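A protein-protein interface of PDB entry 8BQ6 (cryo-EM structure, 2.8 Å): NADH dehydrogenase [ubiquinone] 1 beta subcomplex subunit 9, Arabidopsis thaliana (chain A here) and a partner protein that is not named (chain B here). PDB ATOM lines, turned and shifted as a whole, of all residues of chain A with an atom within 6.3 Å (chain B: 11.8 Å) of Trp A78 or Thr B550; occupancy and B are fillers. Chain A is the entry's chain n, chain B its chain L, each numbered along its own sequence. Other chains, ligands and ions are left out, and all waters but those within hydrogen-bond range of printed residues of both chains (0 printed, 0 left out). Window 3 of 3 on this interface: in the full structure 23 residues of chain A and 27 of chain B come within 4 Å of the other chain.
The guanidinium group (NH1) of Arg B366 sits close to a ring nitrogen (NE2) of His A80 (3.5 Å).
O of Phe B546 sits at hydrogen-bond distance from ND2 of Asn B553 (3.0 Å). SG of Cys B552 is in hydrogen-bond range of OG of Ser B549, 3.6 Å away. The side-chain carboxylate of Glu A74 sits at hydrogen-bond distance from the indole nitrogen of Trp A78 (3.3 Å). The backbone carbonyl oxygen (O) of Trp A78 sits at hydrogen-bond distance from the indole nitrogen (NE1) of Trp A34 (3.2 Å). The side-chain carboxylate of Asp A30 lies within hydrogen-bond range of the backbone NH of His A80.
Phe B546 touches Trp A34 (CD2 to CZ3, 3.7 Å). CD1 of Trp A34 touches NE2 of Gln B547 (3.6 Å). CZ3 of Trp A34 touches CD2 of Tyr B556, 3.6 Å away. Asn B553 touches Lys A77 (OD1 to O, 3.96 Å). Trp A78 touches Phe B546 (CZ3 to O, 3.2 Å). Gln B547 touches Trp A78. Trp A78 touches Thr B548 (CH2 to C, 3.3 Å). Ser B549 touches Trp A78 (O to CZ3, 3.5 Å). CH2 of Trp A78 touches N of Thr B550, 3.7 Å away. CB of Asn B553 touches CZ3 of Trp A78 (3.8 Å).
No residue of chain B comes within 4 Å of Glu A74. Printed residues of chain B within 4 Å of Lys A77: Asn B553 (3.96 Å). Trp A78 touches just these residues of chain B: Phe B546, Gln B547, Thr B548, Ser B549, Thr B550 and Asn B553. Of the printed residues of chain A, Gln B543 touches Trp A34. Thr B550 touches just one residue of chain A: Trp A78. Printed residues of chain A within 4 Å of Tyr B556: Trp A34. The nearest residue of chain B that does not touch Trp A78 is Ala B545 (5.6 Å). The nearest printed residue of chain A that does not touch Thr B550 is Lys A77 (7.4 Å).
Hydrophobic or aromatic side chains of chain A that line the printed part of chain B: Trp A34, Trp A78 and His A80. Of the 21 printed residues of chain B, 9 touch a printed residue of chain A. Among the printed residues, no Asp or Glu carboxylate lies within 4 Å of a Lys or Arg side-chain nitrogen of the other chain.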
ATOM      1  N   ASP A  30      10.810  10.939  -6.856  1.00  0.00           N
ATOM      2  CA  ASP A  30      10.324  12.118  -7.564  1.00  0.00           C
ATOM      3  C   ASP A  30      11.225  12.489  -8.731  1.00  0.00           C
ATOM      4  O   ASP A  30      10.795  13.201  -9.645  1.00  0.00           O
ATOM      5  CB  ASP A  30      10.197  13.301  -6.612  1.00  0.00           C
ATOM      6  CG  ASP A  30       9.087  14.242  -7.013  1.00  0.00           C
ATOM      7  OD1 ASP A  30       7.980  13.756  -7.326  1.00  0.00           O
ATOM      8  OD2 ASP A  30       9.326  15.465  -7.039  1.00  0.00           O
ATOM      9  N   TRP A  34       9.994  13.266 -12.885  1.00  0.00           N
ATOM     10  CA  TRP A  34      10.364  14.405 -13.759  1.00  0.00           C
ATOM     11  C   TRP A  34      11.101  13.898 -14.997  1.00  0.00           C
ATOM     12  O   TRP A  34      11.053  14.600 -16.009  1.00  0.00           O
ATOM     13  CB  TRP A  34      11.240  15.384 -12.974  1.00  0.00           C
ATOM     14  CG  TRP A  34      10.504  16.326 -12.076  1.00  0.00           C
ATOM     15  CD1 TRP A  34      10.491  16.318 -10.713  1.00  0.00           C
ATOM     16  CD2 TRP A  34       9.701  17.448 -12.478  1.00  0.00           C
ATOM     17  NE1 TRP A  34       9.727  17.349 -10.239  1.00  0.00           N
ATOM     18  CE2 TRP A  34       9.228  18.058 -11.298  1.00  0.00           C
ATOM     19  CE3 TRP A  34       9.329  17.988 -13.714  1.00  0.00           C
ATOM     20  CZ2 TRP A  34       8.399  19.177 -11.321  1.00  0.00           C
ATOM     21  CZ3 TRP A  34       8.511  19.094 -13.733  1.00  0.00           C
ATOM     22  CH2 TRP A  34       8.054  19.679 -12.554  1.00  0.00           C
ATOM     23  N   ALA A  73      12.524  21.344   2.612  1.00  0.00           N
ATOM     24  CA  ALA A  73      11.993  22.507   1.907  1.00  0.00           C
ATOM     25  C   ALA A  73      12.222  22.396   0.408  1.00  0.00           C
ATOM     26  O   ALA A  73      11.357  22.774  -0.392  1.00  0.00           O
ATOM     27  CB  ALA A  73      12.630  23.789   2.440  1.00  0.00           C
ATOM     28  N   GLU A  74      13.396  21.909   0.010  1.00  0.00           N
ATOM     29  CA  GLU A  74      13.684  21.737  -1.409  1.00  0.00           C
ATOM     30  C   GLU A  74      12.782  20.679  -2.027  1.00  0.00           C
ATOM     31  O   GLU A  74      12.282  20.848  -3.145  1.00  0.00           O
ATOM     32  CB  GLU A  74      15.154  21.375  -1.594  1.00  0.00           C
ATOM     33  CG  GLU A  74      16.084  22.518  -1.263  1.00  0.00           C
ATOM     34  CD  GLU A  74      15.571  23.842  -1.785  1.00  0.00           C
ATOM     35  OE1 GLU A  74      15.797  24.129  -2.977  1.00  0.00           O
ATOM     36  OE2 GLU A  74      14.934  24.589  -1.009  1.00  0.00           O
ATOM     37  N   TYR A  75      12.573  19.568  -1.318  1.00  0.00           N
ATOM     38  CA  TYR A  75      11.698  18.524  -1.835  1.00  0.00           C
ATOM     39  C   TYR A  75      10.260  19.016  -1.944  1.00  0.00           C
ATOM     40  O   TYR A  75       9.584  18.772  -2.948  1.00  0.00           O
ATOM     41  CB  TYR A  75      11.775  17.278  -0.951  1.00  0.00           C
ATOM     42  CG  TYR A  75      10.713  16.258  -1.280  1.00  0.00           C
ATOM     43  CD1 TYR A  75      10.833  15.435  -2.390  1.00  0.00           C
ATOM     44  CD2 TYR A  75       9.584  16.124  -0.485  1.00  0.00           C
ATOM     45  CE1 TYR A  75       9.859  14.507  -2.696  1.00  0.00           C
ATOM     46  CE2 TYR A  75       8.607  15.201  -0.784  1.00  0.00           C
ATOM     47  CZ  TYR A  75       8.748  14.395  -1.889  1.00  0.00           C
ATOM     48  OH  TYR A  75       7.766  13.477  -2.182  1.00  0.00           O
ATOM     49  N   ASN A  76       9.779  19.726  -0.919  1.00  0.00           N
ATOM     50  CA  ASN A  76       8.400  20.206  -0.936  1.00  0.00           C
ATOM     51  C   ASN A  76       8.197  21.311  -1.963  1.00  0.00           C
ATOM     52  O   ASN A  76       7.065  21.554  -2.394  1.00  0.00           O
ATOM     53  CB  ASN A  76       7.995  20.701   0.451  1.00  0.00           C
ATOM     54  CG  ASN A  76       7.818  19.574   1.444  1.00  0.00           C
ATOM     55  OD1 ASN A  76       7.324  18.500   1.101  1.00  0.00           O
ATOM     56  ND2 ASN A  76       8.222  19.811   2.687  1.00  0.00           N
ATOM     57  N   LYS A  77       9.270  21.995  -2.359  1.00  0.00           N
ATOM     58  CA  LYS A  77       9.140  23.063  -3.343  1.00  0.00           C
ATOM     59  C   LYS A  77       9.196  22.524  -4.767  1.00  0.00           C
ATOM     60  O   LYS A  77       8.341  22.854  -5.595  1.00  0.00           O
ATOM     61  CB  LYS A  77      10.230  24.112  -3.125  1.00  0.00           C
ATOM     62  CG  LYS A  77      10.080  24.876  -1.826  1.00  0.00           C
ATOM     63  CD  LYS A  77      11.193  25.881  -1.646  1.00  0.00           C
ATOM     64  CE  LYS A  77      11.011  26.652  -0.353  1.00  0.00           C
ATOM     65  NZ  LYS A  77      12.114  27.628  -0.155  1.00  0.00           N
ATOM     66  N   TRP A  78      10.194  21.696  -5.071  1.00  0.00           N
ATOM     67  CA  TRP A  78      10.406  21.181  -6.418  1.00  0.00           C
ATOM     68  C   TRP A  78       9.759  19.821  -6.642  1.00  0.00           C
ATOM     69  O   TRP A  78      10.171  19.096  -7.553  1.00  0.00           O
ATOM     70  CB  TRP A  78      11.905  21.090  -6.718  1.00  0.00           C
ATOM     71  CG  TRP A  78      12.619  22.377  -6.527  1.00  0.00           C
ATOM     72  CD1 TRP A  78      13.439  22.709  -5.492  1.00  0.00           C
ATOM     73  CD2 TRP A  78      12.590  23.511  -7.399  1.00  0.00           C
ATOM     74  NE1 TRP A  78      13.918  23.985  -5.659  1.00  0.00           N
ATOM     75  CE2 TRP A  78      13.414  24.498  -6.824  1.00  0.00           C
ATOM     76  CE3 TRP A  78      11.950  23.787  -8.609  1.00  0.00           C
ATOM     77  CZ2 TRP A  78      13.610  25.743  -7.416  1.00  0.00           C
ATOM     78  CZ3 TRP A  78      12.147  25.023  -9.197  1.00  0.00           C
ATOM     79  CH2 TRP A  78      12.970  25.986  -8.600  1.00  0.00           C
ATOM     80  N   ARG A  79       8.769  19.463  -5.826  1.00  0.00           N
ATOM     81  CA  ARG A  79       8.082  18.185  -5.950  1.00  0.00           C
ATOM     82  C   ARG A  79       7.268  18.143  -7.237  1.00  0.00           C
ATOM     83  O   ARG A  79       6.776  19.169  -7.712  1.00  0.00           O
ATOM     84  CB  ARG A  79       7.174  17.975  -4.730  1.00  0.00           C
ATOM     85  CG  ARG A  79       6.631  16.566  -4.518  1.00  0.00           C
ATOM     86  CD  ARG A  79       5.198  16.596  -3.974  1.00  0.00           C
ATOM     87  NE  ARG A  79       4.998  15.704  -2.835  1.00  0.00           N
ATOM     88  CZ  ARG A  79       4.629  14.432  -2.924  1.00  0.00           C
ATOM     89  NH1 ARG A  79       4.392  13.859  -4.093  1.00  0.00           N
ATOM     90  NH2 ARG A  79       4.498  13.716  -1.811  1.00  0.00           N
ATOM     91  N   HIS A  80       7.127  16.951  -7.806  1.00  0.00           N
ATOM     92  CA  HIS A  80       6.336  16.800  -9.023  1.00  0.00           C
ATOM     93  C   HIS A  80       4.850  16.935  -8.707  1.00  0.00           C
ATOM     94  O   HIS A  80       4.346  16.244  -7.814  1.00  0.00           O
ATOM     95  CB  HIS A  80       6.612  15.456  -9.687  1.00  0.00           C
ATOM     96  CG  HIS A  80       6.179  15.392 -11.119  1.00  0.00           C
ATOM     97  ND1 HIS A  80       4.857  15.459 -11.498  1.00  0.00           N
ATOM     98  CD2 HIS A  80       6.894  15.286 -12.264  1.00  0.00           C
ATOM     99  CE1 HIS A  80       4.774  15.385 -12.815  1.00  0.00           C
ATOM    100  NE2 HIS A  80       5.995  15.280 -13.303  1.00  0.00           N
ATOM    101  N   ARG B 366       3.773   7.298 -18.232  1.00  0.00           N
ATOM    102  CA  ARG B 366       5.190   7.236 -17.905  1.00  0.00           C
ATOM    103  C   ARG B 366       5.656   5.827 -17.565  1.00  0.00           C
ATOM    104  O   ARG B 366       6.867   5.599 -17.490  1.00  0.00           O
ATOM    105  CB  ARG B 366       5.502   8.178 -16.746  1.00  0.00           C
ATOM    106  CG  ARG B 366       5.061   9.605 -16.977  1.00  0.00           C
ATOM    107  CD  ARG B 366       5.221  10.412 -15.707  1.00  0.00           C
ATOM    108  NE  ARG B 366       4.083  10.234 -14.816  1.00  0.00           N
ATOM    109  CZ  ARG B 366       3.760  11.070 -13.840  1.00  0.00           C
ATOM    110  NH1 ARG B 366       4.504  12.126 -13.560  1.00  0.00           N
ATOM    111  NH2 ARG B 366       2.663  10.837 -13.124  1.00  0.00           N
ATOM    112  N   PHE B 542      15.726  19.202 -20.915  1.00  0.00           N
ATOM    113  CA  PHE B 542      14.507  20.057 -20.942  1.00  0.00           C
ATOM    114  C   PHE B 542      13.806  20.090 -19.571  1.00  0.00           C
ATOM    115  O   PHE B 542      13.489  21.191 -19.093  1.00  0.00           O
ATOM    116  CB  PHE B 542      13.560  19.558 -22.036  1.00  0.00           C
ATOM    117  CG  PHE B 542      12.270  20.323 -22.185  1.00  0.00           C
ATOM    118  CD1 PHE B 542      12.259  21.594 -22.736  1.00  0.00           C
ATOM    119  CD2 PHE B 542      11.063  19.761 -21.801  1.00  0.00           C
ATOM    120  CE1 PHE B 542      11.070  22.293 -22.881  1.00  0.00           C
ATOM    121  CE2 PHE B 542       9.875  20.458 -21.952  1.00  0.00           C
ATOM    122  CZ  PHE B 542       9.881  21.723 -22.491  1.00  0.00           C
ATOM    123  N   GLN B 543      13.542  18.918 -18.979  1.00  0.00           N
ATOM    124  CA  GLN B 543      12.871  18.863 -17.650  1.00  0.00           C
ATOM    125  C   GLN B 543      13.681  19.664 -16.624  1.00  0.00           C
ATOM    126  O   GLN B 543      13.053  20.194 -15.685  1.00  0.00           O
ATOM    127  CB  GLN B 543      12.668  17.409 -17.213  1.00  0.00           C
ATOM    128  CG  GLN B 543      13.942  16.659 -16.843  1.00  0.00           C
ATOM    129  CD  GLN B 543      14.764  16.261 -18.043  1.00  0.00           C
ATOM    130  OE1 GLN B 543      14.407  16.532 -19.186  1.00  0.00           O
ATOM    131  NE2 GLN B 543      15.888  15.614 -17.789  1.00  0.00           N
ATOM    132  N   ARG B 544      15.003  19.791 -16.809  1.00  0.00           N
ATOM    133  CA  ARG B 544      15.847  20.458 -15.776  1.00  0.00           C
ATOM    134  C   ARG B 544      15.425  21.923 -15.631  1.00  0.00           C
ATOM    135  O   ARG B 544      15.564  22.430 -14.519  1.00  0.00           O
ATOM    136  CB  ARG B 544      17.342  20.291 -16.062  1.00  0.00           C
ATOM    137  CG  ARG B 544      17.833  18.857 -15.935  1.00  0.00           C
ATOM    138  CD  ARG B 544      19.324  18.730 -16.176  1.00  0.00           C
ATOM    139  NE  ARG B 544      19.783  17.349 -16.124  1.00  0.00           N
ATOM    140  CZ  ARG B 544      21.018  16.951 -16.412  1.00  0.00           C
ATOM    141  NH1 ARG B 544      21.933  17.830 -16.776  1.00  0.00           N
ATOM    142  NH2 ARG B 544      21.335  15.671 -16.329  1.00  0.00           N
ATOM    143  N   ALA B 545      14.893  22.546 -16.688  1.00  0.00           N
ATOM    144  CA  ALA B 545      14.385  23.937 -16.589  1.00  0.00           C
ATOM    145  C   ALA B 545      13.416  24.055 -15.410  1.00  0.00           C
ATOM    146  O   ALA B 545      13.580  24.985 -14.616  1.00  0.00           O
ATOM    147  CB  ALA B 545      13.713  24.343 -17.879  1.00  0.00           C
ATOM    148  N   PHE B 546      12.450  23.140 -15.303  1.00  0.00           N
ATOM    149  CA  PHE B 546      11.425  23.209 -14.225  1.00  0.00           C
ATOM    150  C   PHE B 546      12.032  22.844 -12.867  1.00  0.00           C
ATOM    151  O   PHE B 546      11.541  23.379 -11.867  1.00  0.00           O
ATOM    152  CB  PHE B 546      10.240  22.288 -14.519  1.00  0.00           C
ATOM    153  CG  PHE B 546       9.843  22.175 -15.968  1.00  0.00           C
ATOM    154  CD1 PHE B 546       9.431  23.287 -16.685  1.00  0.00           C
ATOM    155  CD2 PHE B 546       9.875  20.951 -16.616  1.00  0.00           C
ATOM    156  CE1 PHE B 546       9.069  23.179 -18.017  1.00  0.00           C
ATOM    157  CE2 PHE B 546       9.512  20.843 -17.949  1.00  0.00           C
ATOM    158  CZ  PHE B 546       9.108  21.956 -18.646  1.00  0.00           C
ATOM    159  N   GLN B 547      13.041  21.973 -12.816  1.00  0.00           N
ATOM    160  CA  GLN B 547      13.568  21.524 -11.492  1.00  0.00           C
ATOM    161  C   GLN B 547      14.550  22.550 -10.902  1.00  0.00           C
ATOM    162  O   GLN B 547      15.101  22.256  -9.828  1.00  0.00           O
ATOM    163  CB  GLN B 547      14.210  20.141 -11.626  1.00  0.00           C
ATOM    164  CG  GLN B 547      13.210  19.000 -11.694  1.00  0.00           C
ATOM    165  CD  GLN B 547      13.912  17.666 -11.712  1.00  0.00           C
ATOM    166  OE1 GLN B 547      14.392  17.208 -12.746  1.00  0.00           O
ATOM    167  NE2 GLN B 547      13.986  17.029 -10.555  1.00  0.00           N
ATOM    168  N   THR B 548      14.749  23.707 -11.548  1.00  0.00           N
ATOM    169  CA  THR B 548      15.654  24.745 -11.075  1.00  0.00           C
ATOM    170  C   THR B 548      15.095  26.157 -11.180  1.00  0.00           C
ATOM    171  O   THR B 548      15.602  27.047 -10.490  1.00  0.00           O
ATOM    172  CB  THR B 548      16.989  24.699 -11.839  1.00  0.00           C
ATOM    173  OG1 THR B 548      17.865  25.709 -11.328  1.00  0.00           O
ATOM    174  CG2 THR B 548      16.772  24.980 -13.308  1.00  0.00           C
ATOM    175  N   SER B 549      14.074  26.389 -12.001  1.00  0.00           N
ATOM    176  CA  SER B 549      13.523  27.722 -12.222  1.00  0.00           C
ATOM    177  C   SER B 549      12.134  27.815 -11.606  1.00  0.00           C
ATOM    178  O   SER B 549      11.260  26.996 -11.912  1.00  0.00           O
ATOM    179  CB  SER B 549      13.463  28.047 -13.715  1.00  0.00           C
ATOM    180  OG  SER B 549      12.815  29.285 -13.948  1.00  0.00           O
ATOM    181  N   THR B 550      11.934  28.819 -10.746  1.00  0.00           N
ATOM    182  CA  THR B 550      10.661  28.962 -10.044  1.00  0.00           C
ATOM    183  C   THR B 550       9.521  29.305 -10.998  1.00  0.00           C
ATOM    184  O   THR B 550       8.430  28.733 -10.892  1.00  0.00           O
ATOM    185  CB  THR B 550      10.782  30.019  -8.941  1.00  0.00           C
ATOM    186  OG1 THR B 550       9.828  29.744  -7.908  1.00  0.00           O
ATOM    187  CG2 THR B 550      10.537  31.423  -9.471  1.00  0.00           C
ATOM    188  N   PHE B 551       9.744  30.230 -11.934  1.00  0.00           N
ATOM    189  CA  PHE B 551       8.675  30.596 -12.850  1.00  0.00           C
ATOM    190  C   PHE B 551       8.331  29.438 -13.771  1.00  0.00           C
ATOM    191  O   PHE B 551       7.154  29.197 -14.055  1.00  0.00           O
ATOM    192  CB  PHE B 551       9.059  31.836 -13.654  1.00  0.00           C
ATOM    193  CG  PHE B 551       7.942  32.361 -14.513  1.00  0.00           C
ATOM    194  CD1 PHE B 551       7.170  33.429 -14.097  1.00  0.00           C
ATOM    195  CD2 PHE B 551       7.674  31.790 -15.747  1.00  0.00           C
ATOM    196  CE1 PHE B 551       6.143  33.905 -14.887  1.00  0.00           C
ATOM    197  CE2 PHE B 551       6.652  32.262 -16.535  1.00  0.00           C
ATOM    198  CZ  PHE B 551       5.888  33.322 -16.108  1.00  0.00           C
ATOM    199  N   CYS B 552       9.341  28.714 -14.257  1.00  0.00           N
ATOM    200  CA  CYS B 552       9.064  27.594 -15.150  1.00  0.00           C
ATOM    201  C   CYS B 552       8.437  26.424 -14.402  1.00  0.00           C
ATOM    202  O   CYS B 552       7.746  25.597 -15.006  1.00  0.00           O
ATOM    203  CB  CYS B 552      10.341  27.144 -15.859  1.00  0.00           C
ATOM    204  SG  CYS B 552      11.044  28.354 -16.995  1.00  0.00           S
ATOM    205  N   ASN B 553       8.685  26.322 -13.093  1.00  0.00           N
ATOM    206  CA  ASN B 553       8.075  25.248 -12.317  1.00  0.00           C
ATOM    207  C   ASN B 553       6.601  25.528 -12.049  1.00  0.00           C
ATOM    208  O   ASN B 553       5.763  24.624 -12.149  1.00  0.00           O
ATOM    209  CB  ASN B 553       8.838  25.046 -11.010  1.00  0.00           C
ATOM    210  CG  ASN B 553       8.398  23.803 -10.269  1.00  0.00           C
ATOM    211  OD1 ASN B 553       7.591  23.871  -9.345  1.00  0.00           O
ATOM    212  ND2 ASN B 553       8.912  22.653 -10.687  1.00  0.00           N
ATOM    213  N   ARG B 554       6.266  26.776 -11.707  1.00  0.00           N
ATOM    214  CA  ARG B 554       4.865  27.148 -11.528  1.00  0.00           C
ATOM    215  C   ARG B 554       4.101  27.038 -12.839  1.00  0.00           C
ATOM    216  O   ARG B 554       2.918  26.682 -12.852  1.00  0.00           O
ATOM    217  CB  ARG B 554       4.761  28.572 -10.981  1.00  0.00           C
ATOM    218  CG  ARG B 554       5.235  28.778  -9.547  1.00  0.00           C
ATOM    219  CD  ARG B 554       5.184  27.510  -8.711  1.00  0.00           C
ATOM    220  NE  ARG B 554       4.996  27.816  -7.298  1.00  0.00           N
ATOM    221  CZ  ARG B 554       4.571  26.949  -6.389  1.00  0.00           C
ATOM    222  NH1 ARG B 554       4.268  25.702  -6.710  1.00  0.00           N
ATOM    223  NH2 ARG B 554       4.446  27.344  -5.125  1.00  0.00           N
ATOM    224  N   LEU B 555       4.762  27.358 -13.949  1.00  0.00           N
ATOM    225  CA  LEU B 555       4.132  27.244 -15.258  1.00  0.00           C
ATOM    226  C   LEU B 555       3.780  25.796 -15.580  1.00  0.00           C
ATOM    227  O   LEU B 555       2.721  25.520 -16.157  1.00  0.00           O
ATOM    228  CB  LEU B 555       5.061  27.831 -16.316  1.00  0.00           C
ATOM    229  CG  LEU B 555       4.407  28.375 -17.578  1.00  0.00           C
ATOM    230  CD1 LEU B 555       5.308  29.407 -18.205  1.00  0.00           C
ATOM    231  CD2 LEU B 555       4.171  27.243 -18.543  1.00  0.00           C
ATOM    232  N   TYR B 556       4.669  24.860 -15.238  1.00  0.00           N
ATOM    233  CA  TYR B 556       4.373  23.442 -15.421  1.00  0.00           C
ATOM    234  C   TYR B 556       3.158  23.031 -14.606  1.00  0.00           C
ATOM    235  O   TYR B 556       2.304  22.269 -15.074  1.00  0.00           O
ATOM    236  CB  TYR B 556       5.576  22.596 -15.008  1.00  0.00           C
ATOM    237  CG  TYR B 556       5.560  21.188 -15.556  1.00  0.00           C
ATOM    238  CD1 TYR B 556       5.892  20.934 -16.875  1.00  0.00           C
ATOM    239  CD2 TYR B 556       5.179  20.117 -14.759  1.00  0.00           C
ATOM    240  CE1 TYR B 556       5.877  19.651 -17.378  1.00  0.00           C
ATOM    241  CE2 TYR B 556       5.155  18.829 -15.258  1.00  0.00           C
ATOM    242  CZ  TYR B 556       5.505  18.603 -16.568  1.00  0.00           C
ATOM    243  OH  TYR B 556       5.486  17.324 -17.072  1.00  0.00           O
ATOM    244  N   SER B 557       3.080  23.510 -13.367  1.00  0.00           N
ATOM    245  CA  SER B 557       1.957  23.159 -12.509  1.00  0.00           C
ATOM    246  C   SER B 557       0.695  23.900 -12.931  1.00  0.00           C
ATOM    247  O   SER B 557      -0.422  23.418 -12.717  1.00  0.00           O
ATOM    248  CB  SER B 557       2.311  23.451 -11.051  1.00  0.00           C
ATOM    249  OG  SER B 557       1.870  24.740 -10.665  1.00  0.00           O
ATOM    250  N   PHE B 558       0.855  25.072 -13.547  1.00  0.00           N
ATOM    251  CA  PHE B 558      -0.305  25.824 -14.014  1.00  0.00           C
ATOM    252  C   PHE B 558      -1.080  25.049 -15.074  1.00  0.00           C
ATOM    253  O   PHE B 558      -2.310  24.946 -15.011  1.00  0.00           O
ATOM    254  CB  PHE B 558       0.138  27.185 -14.550  1.00  0.00           C
ATOM    255  CG  PHE B 558      -0.975  27.983 -15.153  1.00  0.00           C
ATOM    256  CD1 PHE B 558      -1.850  28.688 -14.350  1.00  0.00           C
ATOM    257  CD2 PHE B 558      -1.146  28.029 -16.525  1.00  0.00           C
ATOM    258  CE1 PHE B 558      -2.877  29.420 -14.900  1.00  0.00           C
ATOM    259  CE2 PHE B 558      -2.172  28.758 -17.081  1.00  0.00           C
ATOM    260  CZ  PHE B 558      -3.037  29.456 -16.268  1.00  0.00           C
ATOM    261  N   PHE B 559      -0.373  24.488 -16.056  1.00  0.00           N
ATOM    262  CA  PHE B 559      -1.041  23.740 -17.117  1.00  0.00           C
ATOM    263  C   PHE B 559      -1.333  22.303 -16.713  1.00  0.00           C
ATOM    264  O   PHE B 559      -2.187  21.653 -17.326  1.00  0.00           O
ATOM    265  CB  PHE B 559      -0.193  23.761 -18.386  1.00  0.00           C
ATOM    266  CG  PHE B 559      -0.236  25.065 -19.115  1.00  0.00           C
ATOM    267  CD1 PHE B 559      -1.440  25.592 -19.545  1.00  0.00           C
ATOM    268  CD2 PHE B 559       0.924  25.773 -19.358  1.00  0.00           C
ATOM    269  CE1 PHE B 559      -1.482  26.797 -20.215  1.00  0.00           C
ATOM    270  CE2 PHE B 559       0.887  26.978 -20.027  1.00  0.00           C
ATOM    271  CZ  PHE B 559      -0.318  27.491 -20.454  1.00  0.00           C
ATOM    272  N   LYS B 561      -2.315  21.494 -13.519  1.00  0.00           N
ATOM    273  CA  LYS B 561      -3.467  21.588 -12.580  1.00  0.00           C
ATOM    274  C   LYS B 561      -4.619  22.379 -13.212  1.00  0.00           C
ATOM    275  O   LYS B 561      -5.396  22.965 -12.438  1.00  0.00           O
ATOM    276  CB  LYS B 561      -3.015  22.183 -11.241  1.00  0.00           C
ATOM    277  CG  LYS B 561      -2.041  21.312 -10.458  1.00  0.00           C
ATOM    278  CD  LYS B 561      -1.625  21.907  -9.131  1.00  0.00           C
ATOM    279  CE  LYS B 561      -0.911  20.909  -8.246  1.00  0.00           C
ATOM    280  NZ  LYS B 561      -0.574  21.484  -6.924  1.00  0.00           N
ATOM    281  N   PHE B 564      -5.469  26.105 -12.417  1.00  0.00           N
ATOM    282  CA  PHE B 564      -5.923  26.227 -11.006  1.00  0.00           C
ATOM    283  C   PHE B 564      -7.391  26.658 -10.977  1.00  0.00           C
ATOM    284  O   PHE B 564      -7.727  27.562 -10.205  1.00  0.00           O
ATOM    285  CB  PHE B 564      -5.036  27.194 -10.221  1.00  0.00           C
ATOM    286  CG  PHE B 564      -3.553  26.970 -10.358  1.00  0.00           C
ATOM    287  CD1 PHE B 564      -2.988  25.739 -10.068  1.00  0.00           C
ATOM    288  CD2 PHE B 564      -2.718  28.000 -10.760  1.00  0.00           C
ATOM    289  CE1 PHE B 564      -1.623  25.539 -10.194  1.00  0.00           C
ATOM    290  CE2 PHE B 564      -1.353  27.800 -10.879  1.00  0.00           C
ATOM    291  CZ  PHE B 564      -0.809  26.571 -10.592  1.00  0.00           C
